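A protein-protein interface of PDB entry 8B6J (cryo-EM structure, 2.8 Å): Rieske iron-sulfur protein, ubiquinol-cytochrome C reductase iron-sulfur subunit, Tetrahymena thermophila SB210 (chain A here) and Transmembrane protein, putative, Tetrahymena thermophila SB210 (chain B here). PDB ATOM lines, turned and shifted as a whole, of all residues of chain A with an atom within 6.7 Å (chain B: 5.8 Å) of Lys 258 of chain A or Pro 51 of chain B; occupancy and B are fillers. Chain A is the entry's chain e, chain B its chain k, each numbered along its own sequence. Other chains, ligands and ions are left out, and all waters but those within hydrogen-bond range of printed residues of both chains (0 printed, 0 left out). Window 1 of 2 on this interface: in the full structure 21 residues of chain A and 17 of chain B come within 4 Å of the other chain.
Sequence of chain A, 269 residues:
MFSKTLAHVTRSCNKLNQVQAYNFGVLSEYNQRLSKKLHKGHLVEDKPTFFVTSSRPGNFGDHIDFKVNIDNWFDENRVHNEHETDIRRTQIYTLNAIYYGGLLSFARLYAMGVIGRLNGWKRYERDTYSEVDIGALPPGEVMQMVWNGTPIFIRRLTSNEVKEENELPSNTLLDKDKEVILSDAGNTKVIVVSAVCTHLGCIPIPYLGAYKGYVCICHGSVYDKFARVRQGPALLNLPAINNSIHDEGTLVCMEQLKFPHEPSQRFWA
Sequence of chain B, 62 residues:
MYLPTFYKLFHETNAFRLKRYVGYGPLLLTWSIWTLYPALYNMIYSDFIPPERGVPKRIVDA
Among the printed residues, merely in contact across the chains: Asn 242 of chain A with Arg 53 of chain B, Leu 257 of chain A with Pro 51 of chain B, Leu 257 of chain A with Glu 52 of chain B, Lys 258 of chain A with Pro 51 of chain B, Phe 259 of chain A with Ser 46 of chain B, Phe 259 of chain A with Pro 51 of chain B and Pro 260 of chain A with Tyr 45 of chain B.
Printed residues of chain B that touch a printed residue of chain A: Tyr 45, Ser 46, Pro 51, Glu 52 and Arg 53. Hydrophobic or aromatic side chains of chain B that line the printed part of chain A: Tyr 45 and Pro 51. Of the 8 printed residues of chain A, 5 touch a printed residue of chain B. Printed residues of chain A that touch a printed residue of chain B: Asn 242, Leu 257, Lys 258, Phe 259 and Pro 260. Hydrophobic or aromatic side chains of chain A within 4 Å of the printed part of chain B: Leu 257, Phe 259 and Pro 260. Among the printed residues, no Asp or Glu carboxylate lies within 4 Å of a Lys or Arg side-chain nitrogen of the other chain.
The side-chain amide nitrogen (ND2) of Asn 242 of chain A is in hydrogen-bond range of the backbone carbonyl oxygen (O) of Glu 255 of chain A (3.2 Å). The side-chain carboxylate (OE2) of Glu 255 of chain A lies within salt-bridge range of the side-chain amino group (NZ) of Lys 258 of chain A, at 3.4 Å.
Of the printed residues of chain B, Asn 242 of chain A touches Arg 53. Lys 258 of chain A touches just one residue of chain B: Pro 51 (3.6 Å). Printed residues of chain B within 4 Å of Phe 259 of chain A: Ser 46 and Pro 51. Pro 51 of chain B touches three residues of chain A. Of the printed residues of chain A, Arg 53 of chain B touches Asn 242 (3.5 Å). The nearest printed residue of chain B that does not touch Lys 258 of chain A is Glu 52 of chain B (6.3 Å). The nearest printed residue of chain A that does not touch Arg 53 of chain B is Leu 257 of chain A (4.3 Å).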
ATOM      1  N   GLU A 125      20.346 -24.643  -6.953  1.00  0.00           N
ATOM      2  CA  GLU A 125      21.437 -24.252  -7.835  1.00  0.00           C
ATOM      3  C   GLU A 125      22.523 -23.572  -7.013  1.00  0.00           C
ATOM      4  O   GLU A 125      22.263 -22.568  -6.342  1.00  0.00           O
ATOM      5  CB  GLU A 125      20.940 -23.322  -8.940  1.00  0.00           C
ATOM      6  CG  GLU A 125      22.031 -22.870  -9.895  1.00  0.00           C
ATOM      7  CD  GLU A 125      21.500 -22.038 -11.042  1.00  0.00           C
ATOM      8  OE1 GLU A 125      20.270 -22.036 -11.258  1.00  0.00           O
ATOM      9  OE2 GLU A 125      22.315 -21.383 -11.726  1.00  0.00           O
ATOM     10  N   ASN A 242      26.930 -16.046 -19.958  1.00  0.00           N
ATOM     11  CA  ASN A 242      25.870 -15.135 -19.550  1.00  0.00           C
ATOM     12  C   ASN A 242      26.424 -14.072 -18.612  1.00  0.00           C
ATOM     13  O   ASN A 242      27.140 -14.381 -17.655  1.00  0.00           O
ATOM     14  CB  ASN A 242      24.747 -15.917 -18.868  1.00  0.00           C
ATOM     15  CG  ASN A 242      23.612 -15.026 -18.415  1.00  0.00           C
ATOM     16  OD1 ASN A 242      23.431 -13.923 -18.928  1.00  0.00           O
ATOM     17  ND2 ASN A 242      22.839 -15.501 -17.447  1.00  0.00           N
ATOM     18  N   GLU A 255      26.827 -14.611 -14.189  1.00  0.00           N
ATOM     19  CA  GLU A 255      26.200 -15.733 -13.510  1.00  0.00           C
ATOM     20  C   GLU A 255      25.785 -16.751 -14.560  1.00  0.00           C
ATOM     21  O   GLU A 255      25.315 -16.377 -15.637  1.00  0.00           O
ATOM     22  CB  GLU A 255      24.985 -15.284 -12.690  1.00  0.00           C
ATOM     23  CG  GLU A 255      24.359 -16.385 -11.852  1.00  0.00           C
ATOM     24  CD  GLU A 255      23.138 -15.911 -11.090  1.00  0.00           C
ATOM     25  OE1 GLU A 255      22.610 -14.831 -11.424  1.00  0.00           O
ATOM     26  OE2 GLU A 255      22.708 -16.618 -10.154  1.00  0.00           O
ATOM     27  N   GLN A 256      25.962 -18.030 -14.243  1.00  0.00           N
ATOM     28  CA  GLN A 256      25.627 -19.077 -15.197  1.00  0.00           C
ATOM     29  C   GLN A 256      24.131 -19.078 -15.481  1.00  0.00           C
ATOM     30  O   GLN A 256      23.310 -18.843 -14.589  1.00  0.00           O
ATOM     31  CB  GLN A 256      26.061 -20.443 -14.664  1.00  0.00           C
ATOM     32  CG  GLN A 256      25.777 -21.593 -15.615  1.00  0.00           C
ATOM     33  CD  GLN A 256      26.353 -22.906 -15.131  1.00  0.00           C
ATOM     34  OE1 GLN A 256      27.244 -22.930 -14.283  1.00  0.00           O
ATOM     35  NE2 GLN A 256      25.843 -24.008 -15.666  1.00  0.00           N
ATOM     36  N   LEU A 257      23.777 -19.346 -16.735  1.00  0.00           N
ATOM     37  CA  LEU A 257      22.377 -19.367 -17.129  1.00  0.00           C
ATOM     38  C   LEU A 257      21.617 -20.399 -16.307  1.00  0.00           C
ATOM     39  O   LEU A 257      22.063 -21.539 -16.150  1.00  0.00           O
ATOM     40  CB  LEU A 257      22.259 -19.685 -18.620  1.00  0.00           C
ATOM     41  CG  LEU A 257      20.875 -19.515 -19.248  1.00  0.00           C
ATOM     42  CD1 LEU A 257      20.425 -18.066 -19.171  1.00  0.00           C
ATOM     43  CD2 LEU A 257      20.885 -19.998 -20.688  1.00  0.00           C
ATOM     44  N   LYS A 258      20.462 -19.996 -15.782  1.00  0.00           N
ATOM     45  CA  LYS A 258      19.664 -20.848 -14.908  1.00  0.00           C
ATOM     46  C   LYS A 258      18.663 -21.628 -15.751  1.00  0.00           C
ATOM     47  O   LYS A 258      17.755 -21.043 -16.351  1.00  0.00           O
ATOM     48  CB  LYS A 258      18.952 -20.013 -13.847  1.00  0.00           C
ATOM     49  CG  LYS A 258      19.892 -19.263 -12.921  1.00  0.00           C
ATOM     50  CD  LYS A 258      19.133 -18.576 -11.799  1.00  0.00           C
ATOM     51  CE  LYS A 258      20.077 -17.841 -10.863  1.00  0.00           C
ATOM     52  NZ  LYS A 258      19.352 -17.184  -9.741  1.00  0.00           N
ATOM     53  N   PHE A 259      18.827 -22.945 -15.795  1.00  0.00           N
ATOM     54  CA  PHE A 259      17.878 -23.820 -16.461  1.00  0.00           C
ATOM     55  C   PHE A 259      16.843 -24.329 -15.469  1.00  0.00           C
ATOM     56  O   PHE A 259      17.097 -24.390 -14.263  1.00  0.00           O
ATOM     57  CB  PHE A 259      18.608 -24.995 -17.106  1.00  0.00           C
ATOM     58  CG  PHE A 259      19.363 -24.630 -18.350  1.00  0.00           C
ATOM     59  CD1 PHE A 259      18.697 -24.434 -19.546  1.00  0.00           C
ATOM     60  CD2 PHE A 259      20.738 -24.488 -18.325  1.00  0.00           C
ATOM     61  CE1 PHE A 259      19.386 -24.098 -20.693  1.00  0.00           C
ATOM     62  CE2 PHE A 259      21.433 -24.154 -19.470  1.00  0.00           C
ATOM     63  CZ  PHE A 259      20.756 -23.958 -20.655  1.00  0.00           C
ATOM     64  N   PRO A 260      15.656 -24.704 -15.945  1.00  0.00           N
ATOM     65  CA  PRO A 260      14.609 -25.157 -15.021  1.00  0.00           C
ATOM     66  C   PRO A 260      14.915 -26.545 -14.479  1.00  0.00           C
ATOM     67  O   PRO A 260      15.260 -27.459 -15.229  1.00  0.00           O
ATOM     68  CB  PRO A 260      13.349 -25.156 -15.890  1.00  0.00           C
ATOM     69  CG  PRO A 260      13.855 -25.406 -17.262  1.00  0.00           C
ATOM     70  CD  PRO A 260      15.205 -24.742 -17.346  1.00  0.00           C
ATOM     71  N   TYR B  45      11.534 -26.511 -21.454  1.00  0.00           N
ATOM     72  CA  TYR B  45      12.015 -25.182 -21.103  1.00  0.00           C
ATOM     73  C   TYR B  45      13.525 -25.121 -20.916  1.00  0.00           C
ATOM     74  O   TYR B  45      14.030 -24.139 -20.361  1.00  0.00           O
ATOM     75  CB  TYR B  45      11.305 -24.694 -19.840  1.00  0.00           C
ATOM     76  CG  TYR B  45       9.853 -24.351 -20.071  1.00  0.00           C
ATOM     77  CD1 TYR B  45       8.877 -25.335 -20.065  1.00  0.00           C
ATOM     78  CD2 TYR B  45       9.459 -23.041 -20.306  1.00  0.00           C
ATOM     79  CE1 TYR B  45       7.550 -25.027 -20.280  1.00  0.00           C
ATOM     80  CE2 TYR B  45       8.135 -22.722 -20.522  1.00  0.00           C
ATOM     81  CZ  TYR B  45       7.183 -23.720 -20.508  1.00  0.00           C
ATOM     82  OH  TYR B  45       5.861 -23.408 -20.722  1.00  0.00           O
ATOM     83  N   SER B  46      14.259 -26.137 -21.363  1.00  0.00           N
ATOM     84  CA  SER B  46      15.715 -26.110 -21.364  1.00  0.00           C
ATOM     85  C   SER B  46      16.290 -26.038 -22.769  1.00  0.00           C
ATOM     86  O   SER B  46      17.084 -25.143 -23.068  1.00  0.00           O
ATOM     87  CB  SER B  46      16.265 -27.347 -20.639  1.00  0.00           C
ATOM     88  OG  SER B  46      15.815 -28.541 -21.252  1.00  0.00           O
ATOM     89  N   ILE B  49      12.560 -23.190 -26.151  1.00  0.00           N
ATOM     90  CA  ILE B  49      12.285 -21.980 -25.381  1.00  0.00           C
ATOM     91  C   ILE B  49      13.438 -21.758 -24.408  1.00  0.00           C
ATOM     92  O   ILE B  49      13.234 -21.802 -23.186  1.00  0.00           O
ATOM     93  CB  ILE B  49      10.946 -22.084 -24.632  1.00  0.00           C
ATOM     94  CG1 ILE B  49       9.850 -22.608 -25.564  1.00  0.00           C
ATOM     95  CG2 ILE B  49      10.550 -20.728 -24.064  1.00  0.00           C
ATOM     96  CD1 ILE B  49       8.503 -22.771 -24.895  1.00  0.00           C
ATOM     97  N   PRO B  50      14.655 -21.525 -24.893  1.00  0.00           N
ATOM     98  CA  PRO B  50      15.788 -21.418 -23.983  1.00  0.00           C
ATOM     99  C   PRO B  50      15.638 -20.213 -23.077  1.00  0.00           C
ATOM    100  O   PRO B  50      15.005 -19.207 -23.452  1.00  0.00           O
ATOM    101  CB  PRO B  50      16.988 -21.269 -24.930  1.00  0.00           C
ATOM    102  CG  PRO B  50      16.414 -20.702 -26.180  1.00  0.00           C
ATOM    103  CD  PRO B  50      15.038 -21.283 -26.294  1.00  0.00           C
ATOM    104  N   PRO B  51      16.198 -20.268 -21.868  1.00  0.00           N
ATOM    105  CA  PRO B  51      16.114 -19.110 -20.971  1.00  0.00           C
ATOM    106  C   PRO B  51      16.811 -17.894 -21.563  1.00  0.00           C
ATOM    107  O   PRO B  51      17.793 -18.008 -22.300  1.00  0.00           O
ATOM    108  CB  PRO B  51      16.819 -19.589 -19.696  1.00  0.00           C
ATOM    109  CG  PRO B  51      16.801 -21.071 -19.773  1.00  0.00           C
ATOM    110  CD  PRO B  51      16.875 -21.407 -21.225  1.00  0.00           C
ATOM    111  N   GLU B  52      16.287 -16.717 -21.230  1.00  0.00           N
ATOM    112  CA  GLU B  52      16.890 -15.476 -21.691  1.00  0.00           C
ATOM    113  C   GLU B  52      18.242 -15.258 -21.023  1.00  0.00           C
ATOM    114  O   GLU B  52      18.488 -15.705 -19.900  1.00  0.00           O
ATOM    115  CB  GLU B  52      15.971 -14.292 -21.400  1.00  0.00           C
ATOM    116  CG  GLU B  52      14.683 -14.293 -22.205  1.00  0.00           C
ATOM    117  CD  GLU B  52      13.842 -13.058 -21.954  1.00  0.00           C
ATOM    118  OE1 GLU B  52      14.240 -12.230 -21.108  1.00  0.00           O
ATOM    119  OE2 GLU B  52      12.784 -12.913 -22.603  1.00  0.00           O
ATOM    120  N   ARG B  53      19.126 -14.559 -21.732  1.00  0.00           N
ATOM    121  CA  ARG B  53      20.468 -14.266 -21.235  1.00  0.00           C
ATOM    122  C   ARG B  53      20.426 -12.943 -20.481  1.00  0.00           C
ATOM    123  O   ARG B  53      20.428 -11.868 -21.085  1.00  0.00           O
ATOM    124  CB  ARG B  53      21.471 -14.222 -22.382  1.00  0.00           C
ATOM    125  CG  ARG B  53      21.675 -15.556 -23.074  1.00  0.00           C
ATOM    126  CD  ARG B  53      22.770 -15.473 -24.122  1.00  0.00           C
ATOM    127  NE  ARG B  53      22.989 -16.751 -24.788  1.00  0.00           N
ATOM    128  CZ  ARG B  53      23.910 -16.963 -25.719  1.00  0.00           C
ATOM    129  NH1 ARG B  53      24.723 -16.000 -26.121  1.00  0.00           N
ATOM    130  NH2 ARG B  53      24.017 -18.174 -26.261  1.00  0.00           N
